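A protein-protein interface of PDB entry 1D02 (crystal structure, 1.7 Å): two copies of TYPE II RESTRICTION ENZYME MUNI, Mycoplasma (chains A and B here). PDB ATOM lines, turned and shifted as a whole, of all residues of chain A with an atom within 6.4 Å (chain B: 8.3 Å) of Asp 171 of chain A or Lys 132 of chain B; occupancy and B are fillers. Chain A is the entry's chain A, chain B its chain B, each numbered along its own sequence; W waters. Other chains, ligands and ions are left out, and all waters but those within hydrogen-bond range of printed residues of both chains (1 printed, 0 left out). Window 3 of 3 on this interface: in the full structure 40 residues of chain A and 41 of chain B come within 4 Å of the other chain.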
ATOM      1  N   ILE A 166      19.826 -23.307 -23.855  1.00  0.00           N
ATOM      2  CA  ILE A 166      19.354 -23.553 -22.492  1.00  0.00           C
ATOM      3  C   ILE A 166      20.319 -24.484 -21.769  1.00  0.00           C
ATOM      4  O   ILE A 166      20.580 -24.316 -20.576  1.00  0.00           O
ATOM      5  CB  ILE A 166      17.930 -24.144 -22.519  1.00  0.00           C
ATOM      6  CG1 ILE A 166      16.959 -23.065 -23.037  1.00  0.00           C
ATOM      7  CG2 ILE A 166      17.549 -24.665 -21.162  1.00  0.00           C
ATOM      8  CD1 ILE A 166      15.582 -23.640 -23.571  1.00  0.00           C
ATOM      9  N   THR A 167      20.849 -25.467 -22.484  1.00  0.00           N
ATOM     10  CA  THR A 167      21.803 -26.372 -21.858  1.00  0.00           C
ATOM     11  C   THR A 167      22.985 -25.535 -21.359  1.00  0.00           C
ATOM     12  O   THR A 167      23.415 -25.677 -20.208  1.00  0.00           O
ATOM     13  CB  THR A 167      22.292 -27.435 -22.852  1.00  0.00           C
ATOM     14  OG1 THR A 167      21.173 -28.222 -23.259  1.00  0.00           O
ATOM     15  CG2 THR A 167      23.333 -28.377 -22.205  1.00  0.00           C
ATOM     16  N   PHE A 168      23.485 -24.649 -22.217  1.00  0.00           N
ATOM     17  CA  PHE A 168      24.613 -23.770 -21.868  1.00  0.00           C
ATOM     18  C   PHE A 168      24.292 -22.914 -20.640  1.00  0.00           C
ATOM     19  O   PHE A 168      25.108 -22.810 -19.713  1.00  0.00           O
ATOM     20  CB  PHE A 168      24.923 -22.859 -23.055  1.00  0.00           C
ATOM     21  CG  PHE A 168      26.188 -22.048 -22.912  1.00  0.00           C
ATOM     22  CD1 PHE A 168      27.384 -22.492 -23.478  1.00  0.00           C
ATOM     23  CD2 PHE A 168      26.163 -20.819 -22.270  1.00  0.00           C
ATOM     24  CE1 PHE A 168      28.561 -21.709 -23.411  1.00  0.00           C
ATOM     25  CE2 PHE A 168      27.319 -20.021 -22.188  1.00  0.00           C
ATOM     26  CZ  PHE A 168      28.528 -20.470 -22.765  1.00  0.00           C
ATOM     27  N   TRP A 169      23.122 -22.281 -20.639  1.00  0.00           N
ATOM     28  CA  TRP A 169      22.728 -21.429 -19.502  1.00  0.00           C
ATOM     29  C   TRP A 169      22.778 -22.158 -18.166  1.00  0.00           C
ATOM     30  O   TRP A 169      23.310 -21.642 -17.179  1.00  0.00           O
ATOM     31  CB  TRP A 169      21.284 -20.938 -19.632  1.00  0.00           C
ATOM     32  CG  TRP A 169      20.995 -19.992 -20.728  1.00  0.00           C
ATOM     33  CD1 TRP A 169      21.885 -19.377 -21.572  1.00  0.00           C
ATOM     34  CD2 TRP A 169      19.700 -19.533 -21.100  1.00  0.00           C
ATOM     35  NE1 TRP A 169      21.210 -18.550 -22.450  1.00  0.00           N
ATOM     36  CE2 TRP A 169      19.864 -18.634 -22.178  1.00  0.00           C
ATOM     37  CE3 TRP A 169      18.404 -19.799 -20.626  1.00  0.00           C
ATOM     38  CZ2 TRP A 169      18.783 -18.000 -22.787  1.00  0.00           C
ATOM     39  CZ3 TRP A 169      17.330 -19.175 -21.230  1.00  0.00           C
ATOM     40  CH2 TRP A 169      17.527 -18.284 -22.305  1.00  0.00           C
ATOM     41  N   TYR A 170      22.169 -23.346 -18.124  1.00  0.00           N
ATOM     42  CA  TYR A 170      22.096 -24.090 -16.875  1.00  0.00           C
ATOM     43  C   TYR A 170      23.413 -24.670 -16.365  1.00  0.00           C
ATOM     44  O   TYR A 170      23.543 -24.981 -15.171  1.00  0.00           O
ATOM     45  CB  TYR A 170      21.000 -25.161 -16.960  1.00  0.00           C
ATOM     46  CG  TYR A 170      19.612 -24.562 -16.749  1.00  0.00           C
ATOM     47  CD1 TYR A 170      19.025 -23.743 -17.711  1.00  0.00           C
ATOM     48  CD2 TYR A 170      18.925 -24.758 -15.550  1.00  0.00           C
ATOM     49  CE1 TYR A 170      17.786 -23.127 -17.482  1.00  0.00           C
ATOM     50  CE2 TYR A 170      17.693 -24.148 -15.312  1.00  0.00           C
ATOM     51  CZ  TYR A 170      17.129 -23.336 -16.273  1.00  0.00           C
ATOM     52  OH  TYR A 170      15.901 -22.739 -16.031  1.00  0.00           O
ATOM     53  N   ASP A 171      24.374 -24.829 -17.264  1.00  0.00           N
ATOM     54  CA  ASP A 171      25.698 -25.281 -16.854  1.00  0.00           C
ATOM     55  C   ASP A 171      25.637 -26.527 -15.953  1.00  0.00           C
ATOM     56  O   ASP A 171      25.064 -27.538 -16.359  1.00  0.00           O
ATOM     57  CB  ASP A 171      26.391 -24.093 -16.150  1.00  0.00           C
ATOM     58  CG  ASP A 171      27.894 -24.254 -16.073  1.00  0.00           C
ATOM     59  OD1 ASP A 171      28.543 -24.373 -17.131  1.00  0.00           O
ATOM     60  OD2 ASP A 171      28.430 -24.269 -14.942  1.00  0.00           O
ATOM     61  N   HIS A 172      26.172 -26.470 -14.730  1.00  0.00           N
ATOM     62  CA  HIS A 172      26.136 -27.671 -13.897  1.00  0.00           C
ATOM     63  C   HIS A 172      24.814 -27.984 -13.171  1.00  0.00           C
ATOM     64  O   HIS A 172      24.760 -28.866 -12.309  1.00  0.00           O
ATOM     65  CB  HIS A 172      27.329 -27.655 -12.922  1.00  0.00           C
ATOM     66  CG  HIS A 172      27.254 -26.606 -11.859  1.00  0.00           C
ATOM     67  ND1 HIS A 172      26.645 -26.822 -10.638  1.00  0.00           N
ATOM     68  CD2 HIS A 172      27.760 -25.348 -11.810  1.00  0.00           C
ATOM     69  CE1 HIS A 172      26.787 -25.745  -9.881  1.00  0.00           C
ATOM     70  NE2 HIS A 172      27.459 -24.836 -10.567  1.00  0.00           N
ATOM     71  N   TYR A 173      23.744 -27.273 -13.522  1.00  0.00           N
ATOM     72  CA  TYR A 173      22.433 -27.513 -12.915  1.00  0.00           C
ATOM     73  C   TYR A 173      21.504 -28.067 -13.994  1.00  0.00           C
ATOM     74  O   TYR A 173      20.396 -27.556 -14.198  1.00  0.00           O
ATOM     75  CB  TYR A 173      21.834 -26.217 -12.360  1.00  0.00           C
ATOM     76  CG  TYR A 173      22.653 -25.597 -11.251  1.00  0.00           C
ATOM     77  CD1 TYR A 173      23.483 -24.509 -11.510  1.00  0.00           C
ATOM     78  CD2 TYR A 173      22.598 -26.097  -9.947  1.00  0.00           C
ATOM     79  CE1 TYR A 173      24.236 -23.929 -10.509  1.00  0.00           C
ATOM     80  CE2 TYR A 173      23.358 -25.521  -8.925  1.00  0.00           C
ATOM     81  CZ  TYR A 173      24.168 -24.441  -9.221  1.00  0.00           C
ATOM     82  OH  TYR A 173      24.935 -23.864  -8.246  1.00  0.00           O
ATOM     83  N   GLN A 174      21.935 -29.147 -14.637  1.00  0.00           N
ATOM     84  CA  GLN A 174      21.164 -29.741 -15.724  1.00  0.00           C
ATOM     85  C   GLN A 174      19.847 -30.386 -15.319  1.00  0.00           C
ATOM     86  O   GLN A 174      19.018 -30.683 -16.174  1.00  0.00           O
ATOM     87  CB  GLN A 174      22.028 -30.761 -16.470  1.00  0.00           C
ATOM     88  CG  GLN A 174      23.157 -30.116 -17.279  1.00  0.00           C
ATOM     89  CD  GLN A 174      22.635 -29.146 -18.329  1.00  0.00           C
ATOM     90  OE1 GLN A 174      21.857 -29.532 -19.211  1.00  0.00           O
ATOM     91  NE2 GLN A 174      23.079 -27.876 -18.255  1.00  0.00           N
ATOM     92  N   LEU B  49      30.815 -12.327 -28.097  1.00  0.00           N
ATOM     93  CA  LEU B  49      30.015 -13.463 -27.650  1.00  0.00           C
ATOM     94  C   LEU B  49      29.173 -14.066 -28.781  1.00  0.00           C
ATOM     95  O   LEU B  49      28.151 -14.709 -28.529  1.00  0.00           O
ATOM     96  CB  LEU B  49      29.108 -12.982 -26.501  1.00  0.00           C
ATOM     97  CG  LEU B  49      29.862 -12.537 -25.234  1.00  0.00           C
ATOM     98  CD1 LEU B  49      29.209 -11.299 -24.631  1.00  0.00           C
ATOM     99  CD2 LEU B  49      29.873 -13.685 -24.213  1.00  0.00           C
ATOM    100  N   LEU B  52      28.845 -19.137 -29.139  1.00  0.00           N
ATOM    101  CA  LEU B  52      28.681 -19.779 -27.848  1.00  0.00           C
ATOM    102  C   LEU B  52      28.021 -21.145 -27.750  1.00  0.00           C
ATOM    103  O   LEU B  52      28.450 -22.001 -26.952  1.00  0.00           O
ATOM    104  CB  LEU B  52      27.850 -18.893 -26.916  1.00  0.00           C
ATOM    105  CG  LEU B  52      28.278 -17.495 -26.499  1.00  0.00           C
ATOM    106  CD1 LEU B  52      27.185 -16.929 -25.563  1.00  0.00           C
ATOM    107  CD2 LEU B  52      29.627 -17.567 -25.794  1.00  0.00           C
ATOM    108  N   LEU B 125      21.493 -12.925 -17.996  1.00  0.00           N
ATOM    109  CA  LEU B 125      22.896 -12.672 -17.670  1.00  0.00           C
ATOM    110  C   LEU B 125      23.279 -13.270 -16.324  1.00  0.00           C
ATOM    111  O   LEU B 125      24.461 -13.382 -16.027  1.00  0.00           O
ATOM    112  CB  LEU B 125      23.181 -11.170 -17.681  1.00  0.00           C
ATOM    113  CG  LEU B 125      22.923 -10.496 -19.030  1.00  0.00           C
ATOM    114  CD1 LEU B 125      23.189  -9.003 -18.922  1.00  0.00           C
ATOM    115  CD2 LEU B 125      23.800 -11.139 -20.102  1.00  0.00           C
ATOM    116  N   PHE B 126      22.286 -13.638 -15.519  1.00  0.00           N
ATOM    117  CA  PHE B 126      22.564 -14.259 -14.220  1.00  0.00           C
ATOM    118  C   PHE B 126      22.728 -15.785 -14.315  1.00  0.00           C
ATOM    119  O   PHE B 126      23.068 -16.436 -13.310  1.00  0.00           O
ATOM    120  CB  PHE B 126      21.445 -13.959 -13.211  1.00  0.00           C
ATOM    121  CG  PHE B 126      21.389 -12.523 -12.757  1.00  0.00           C
ATOM    122  CD1 PHE B 126      20.565 -11.602 -13.385  1.00  0.00           C
ATOM    123  CD2 PHE B 126      22.108 -12.108 -11.641  1.00  0.00           C
ATOM    124  CE1 PHE B 126      20.451 -10.286 -12.898  1.00  0.00           C
ATOM    125  CE2 PHE B 126      21.996 -10.813 -11.166  1.00  0.00           C
ATOM    126  CZ  PHE B 126      21.162  -9.906 -11.794  1.00  0.00           C
ATOM    127  N   THR B 127      22.473 -16.372 -15.494  1.00  0.00           N
ATOM    128  CA  THR B 127      22.636 -17.829 -15.616  1.00  0.00           C
ATOM    129  C   THR B 127      24.099 -18.178 -15.399  1.00  0.00           C
ATOM    130  O   THR B 127      24.995 -17.427 -15.799  1.00  0.00           O
ATOM    131  CB  THR B 127      22.216 -18.367 -17.006  1.00  0.00           C
ATOM    132  OG1 THR B 127      22.963 -17.723 -18.048  1.00  0.00           O
ATOM    133  CG2 THR B 127      20.711 -18.134 -17.207  1.00  0.00           C
ATOM    134  N   PRO B 128      24.363 -19.323 -14.758  1.00  0.00           N
ATOM    135  CA  PRO B 128      25.765 -19.681 -14.532  1.00  0.00           C
ATOM    136  C   PRO B 128      26.565 -19.775 -15.821  1.00  0.00           C
ATOM    137  O   PRO B 128      27.747 -19.423 -15.859  1.00  0.00           O
ATOM    138  CB  PRO B 128      25.676 -21.000 -13.753  1.00  0.00           C
ATOM    139  CG  PRO B 128      24.263 -21.538 -14.087  1.00  0.00           C
ATOM    140  CD  PRO B 128      23.443 -20.264 -14.097  1.00  0.00           C
ATOM    141  N   GLY B 129      25.913 -20.223 -16.892  1.00  0.00           N
ATOM    142  CA  GLY B 129      26.582 -20.341 -18.164  1.00  0.00           C
ATOM    143  C   GLY B 129      27.039 -19.022 -18.752  1.00  0.00           C
ATOM    144  O   GLY B 129      28.184 -18.927 -19.211  1.00  0.00           O
ATOM    145  N   LEU B 130      26.168 -18.014 -18.776  1.00  0.00           N
ATOM    146  CA  LEU B 130      26.575 -16.733 -19.337  1.00  0.00           C
ATOM    147  C   LEU B 130      27.520 -16.000 -18.399  1.00  0.00           C
ATOM    148  O   LEU B 130      28.396 -15.271 -18.867  1.00  0.00           O
ATOM    149  CB  LEU B 130      25.356 -15.862 -19.687  1.00  0.00           C
ATOM    150  CG  LEU B 130      24.601 -16.430 -20.922  1.00  0.00           C
ATOM    151  CD1 LEU B 130      23.359 -15.591 -21.202  1.00  0.00           C
ATOM    152  CD2 LEU B 130      25.508 -16.391 -22.158  1.00  0.00           C
ATOM    153  N   LEU B 131      27.356 -16.180 -17.088  1.00  0.00           N
ATOM    154  CA  LEU B 131      28.271 -15.535 -16.147  1.00  0.00           C
ATOM    155  C   LEU B 131      29.697 -16.028 -16.428  1.00  0.00           C
ATOM    156  O   LEU B 131      30.642 -15.230 -16.486  1.00  0.00           O
ATOM    157  CB  LEU B 131      27.892 -15.864 -14.698  1.00  0.00           C
ATOM    158  CG  LEU B 131      26.710 -15.096 -14.111  1.00  0.00           C
ATOM    159  CD1 LEU B 131      26.304 -15.685 -12.760  1.00  0.00           C
ATOM    160  CD2 LEU B 131      27.114 -13.610 -13.943  1.00  0.00           C
ATOM    161  N   LYS B 132      29.856 -17.340 -16.592  1.00  0.00           N
ATOM    162  CA  LYS B 132      31.192 -17.898 -16.873  1.00  0.00           C
ATOM    163  C   LYS B 132      31.737 -17.381 -18.200  1.00  0.00           C
ATOM    164  O   LYS B 132      32.917 -17.009 -18.291  1.00  0.00           O
ATOM    165  CB  LYS B 132      31.160 -19.432 -16.912  1.00  0.00           C
ATOM    166  CG  LYS B 132      31.134 -20.069 -15.526  1.00  0.00           C
ATOM    167  CD  LYS B 132      31.040 -21.594 -15.621  1.00  0.00           C
ATOM    168  CE  LYS B 132      30.995 -22.224 -14.228  1.00  0.00           C
ATOM    169  NZ  LYS B 132      31.024 -23.713 -14.336  1.00  0.00           N
ATOM    170  N   ALA B 133      30.897 -17.343 -19.233  1.00  0.00           N
ATOM    171  CA  ALA B 133      31.360 -16.845 -20.526  1.00  0.00           C
ATOM    172  C   ALA B 133      31.793 -15.364 -20.444  1.00  0.00           C
ATOM    173  O   ALA B 133      32.843 -14.962 -20.986  1.00  0.00           O
ATOM    174  CB  ALA B 133      30.251 -17.010 -21.569  1.00  0.00           C
ATOM    175  N   TYR B 134      30.981 -14.553 -19.766  1.00  0.00           N
ATOM    176  CA  TYR B 134      31.276 -13.127 -19.629  1.00  0.00           C
ATOM    177  C   TYR B 134      32.564 -12.893 -18.842  1.00  0.00           C
ATOM    178  O   TYR B 134      33.403 -12.065 -19.229  1.00  0.00           O
ATOM    179  CB  TYR B 134      30.126 -12.400 -18.920  1.00  0.00           C
ATOM    180  CG  TYR B 134      29.002 -11.940 -19.847  1.00  0.00           C
ATOM    181  CD1 TYR B 134      28.485 -12.774 -20.834  1.00  0.00           C
ATOM    182  CD2 TYR B 134      28.473 -10.657 -19.722  1.00  0.00           C
ATOM    183  CE1 TYR B 134      27.456 -12.327 -21.688  1.00  0.00           C
ATOM    184  CE2 TYR B 134      27.451 -10.211 -20.556  1.00  0.00           C
ATOM    185  CZ  TYR B 134      26.955 -11.048 -21.538  1.00  0.00           C
ATOM    186  OH  TYR B 134      25.991 -10.570 -22.398  1.00  0.00           O
ATOM    187  N   ARG B 135      32.721 -13.620 -17.743  1.00  0.00           N
ATOM    188  CA  ARG B 135      33.938 -13.449 -16.941  1.00  0.00           C
ATOM    189  C   ARG B 135      35.188 -13.908 -17.699  1.00  0.00           C
ATOM    190  O   ARG B 135      36.252 -13.276 -17.594  1.00  0.00           O
ATOM    191  CB  ARG B 135      33.811 -14.190 -15.609  1.00  0.00           C
ATOM    192  CG  ARG B 135      32.808 -13.550 -14.629  1.00  0.00           C
ATOM    193  CD  ARG B 135      33.037 -14.123 -13.236  1.00  0.00           C
ATOM    194  NE  ARG B 135      32.084 -13.674 -12.217  1.00  0.00           N
ATOM    195  CZ  ARG B 135      32.155 -12.530 -11.539  1.00  0.00           C
ATOM    196  NH1 ARG B 135      33.142 -11.643 -11.762  1.00  0.00           N
ATOM    197  NH2 ARG B 135      31.286 -12.313 -10.555  1.00  0.00           N
ATOM    198  N   THR B 136      35.075 -14.981 -18.484  1.00  0.00           N
ATOM    199  CA  THR B 136      36.213 -15.477 -19.263  1.00  0.00           C
ATOM    200  C   THR B 136      36.618 -14.489 -20.345  1.00  0.00           C
ATOM    201  O   THR B 136      37.798 -14.159 -20.515  1.00  0.00           O
ATOM    202  CB  THR B 136      35.885 -16.821 -19.969  1.00  0.00           C
ATOM    203  OG1 THR B 136      35.691 -17.830 -18.983  1.00  0.00           O
ATOM    204  CG2 THR B 136      37.016 -17.227 -20.947  1.00  0.00           C
ATOM    205  N   ILE B 137      35.623 -13.986 -21.069  1.00  0.00           N
ATOM    206  CA  ILE B 137      35.914 -13.085 -22.169  1.00  0.00           C
ATOM    207  C   ILE B 137      36.318 -11.692 -21.706  1.00  0.00           C
ATOM    208  O   ILE B 137      37.348 -11.175 -22.129  1.00  0.00           O
ATOM    209  CB  ILE B 137      34.697 -13.017 -23.122  1.00  0.00           C
ATOM    210  CG1 ILE B 137      34.499 -14.391 -23.760  1.00  0.00           C
ATOM    211  CG2 ILE B 137      34.937 -11.954 -24.239  1.00  0.00           C
ATOM    212  CD1 ILE B 137      33.194 -14.558 -24.535  1.00  0.00           C
ATOM    213  N   GLY B 138      35.545 -11.114 -20.796  1.00  0.00           N
ATOM    214  CA  GLY B 138      35.829  -9.764 -20.347  1.00  0.00           C
ATOM    215  C   GLY B 138      36.983  -9.620 -19.376  1.00  0.00           C
ATOM    216  O   GLY B 138      37.500  -8.513 -19.207  1.00  0.00           O
ATOM    217  N   GLY B 139      37.368 -10.712 -18.708  1.00  0.00           N
ATOM    218  CA  GLY B 139      38.488 -10.635 -17.784  1.00  0.00           C
ATOM    219  C   GLY B 139      38.182 -10.216 -16.355  1.00  0.00           C
ATOM    220  O   GLY B 139      39.113 -10.066 -15.562  1.00  0.00           O
ATOM    221  N   ILE B 140      36.904 -10.036 -16.003  1.00  0.00           N
ATOM    222  CA  ILE B 140      36.517  -9.612 -14.660  1.00  0.00           C
ATOM    223  C   ILE B 140      36.147 -10.799 -13.777  1.00  0.00           C
ATOM    224  O   ILE B 140      35.043 -11.336 -13.884  1.00  0.00           O
ATOM    225  CB  ILE B 140      35.299  -8.635 -14.710  1.00  0.00           C
ATOM    226  CG1 ILE B 140      35.619  -7.472 -15.659  1.00  0.00           C
ATOM    227  CG2 ILE B 140      34.948  -8.115 -13.290  1.00  0.00           C
ATOM    228  CD1 ILE B 140      34.410  -6.570 -15.950  1.00  0.00           C
ATOM    229  N   ASN B 141      37.059 -11.211 -12.894  1.00  0.00           N
ATOM    230  CA  ASN B 141      36.779 -12.322 -11.995  1.00  0.00           C
ATOM    231  C   ASN B 141      36.492 -11.914 -10.549  1.00  0.00           C
ATOM    232  O   ASN B 141      36.267 -12.783  -9.691  1.00  0.00           O
ATOM    233  CB  ASN B 141      37.927 -13.346 -12.049  1.00  0.00           C
ATOM    234  CG  ASN B 141      38.002 -14.039 -13.398  1.00  0.00           C
ATOM    235  OD1 ASN B 141      37.028 -14.653 -13.834  1.00  0.00           O
ATOM    236  ND2 ASN B 141      39.146 -13.930 -14.075  1.00  0.00           N
ATOM    237  N   PRO B 147      29.883  -9.393 -14.092  1.00  0.00           N
ATOM    238  CA  PRO B 147      30.538  -8.949 -15.329  1.00  0.00           C
ATOM    239  C   PRO B 147      29.703  -8.189 -16.344  1.00  0.00           C
ATOM    240  O   PRO B 147      30.154  -7.974 -17.465  1.00  0.00           O
ATOM    241  CB  PRO B 147      31.073 -10.254 -15.905  1.00  0.00           C
ATOM    242  CG  PRO B 147      29.974 -11.240 -15.516  1.00  0.00           C
ATOM    243  CD  PRO B 147      29.661 -10.853 -14.092  1.00  0.00           C
HETATM  244  O   HOH W   1      31.184 -24.671 -17.403  1.00  0.00           O
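The backbone NH (N) of Gly 129 of chain B lies within hydrogen-bond range of the backbone carbonyl oxygen (O) of Trp 169 of chain A.
The side-chain amino group of Lys 132 of chain B is in salt-bridge range of the side-chain carboxylate of Asp 171 of chain A (2.7 Å).
O of Asp 171 of chain A sits at hydrogen-bond distance from NE2 of Gln 174 of chain A, 2.8 Å away.
The side-chain hydroxyl (OG1) of Thr 127 of chain B is in hydrogen-bond range of the backbone NH (N) of Leu 130 of chain B, 3.3 Å away.
OG1 of Thr 136 of chain B is in hydrogen-bond range of O of Lys 132 of chain B (3.0 Å).
Among the printed residues, merely in contact across the chains: Trp 169 of chain A with Pro 128 of chain B, Phe 168 of chain A with Gly 129 of chain B, Trp 169 of chain A with Thr 127 of chain B, Phe 168 of chain A with Leu 52 of chain B, Tyr 170 of chain A with Pro 128 of chain B, Trp 169 of chain A with Leu 130 of chain B, Asp 171 of chain A with Pro 128 of chain B and Asp 171 of chain A with Gly 129 of chain B.
Printed residues of chain B within 4 Å of Trp 169 of chain A: Thr 127, Pro 128, Gly 129 and Leu 130.
Asp 171 of chain A touches three residues of chain B.
Of the printed residues of chain A, Pro 128 of chain B touches Trp 169, Tyr 170 and Asp 171.
Of the printed residues of chain A, Gly 129 of chain B touches Phe 168 (3.3 Å), Trp 169 (3.0 Å) and Asp 171 (3.97 Å).
Printed residues of chain A within 4 Å of Leu 130 of chain B: Trp 169.
Lys 132 of chain B touches just one residue of chain A: Asp 171.
The nearest residue of chain B that does not touch Asp 171 of chain A is Thr 127 of chain B (6.4 Å).
The nearest printed residue of chain A that does not touch Thr 127 of chain B is Tyr 170 of chain A (5.1 Å).
Of the 20 printed residues of chain B, 6 touch a printed residue of chain A.
Hydrophobic or aromatic side chains of chain B that line the printed part of chain A: Pro 128 and Leu 130.
Of the 9 printed residues of chain A, 4 touch a printed residue of chain B.
Among the printed residues, Asp or Glu carboxylates within 4 Å of a Lys or Arg side-chain nitrogen of the other chain: Asp 171 of chain A with Lys 132 of chain B.
No position is printed for both chains.
Water W1 bridges OD1 of Asp 171 of chain A (2.7 Å) and NZ of Lys 132 of chain B (3.2 Å).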
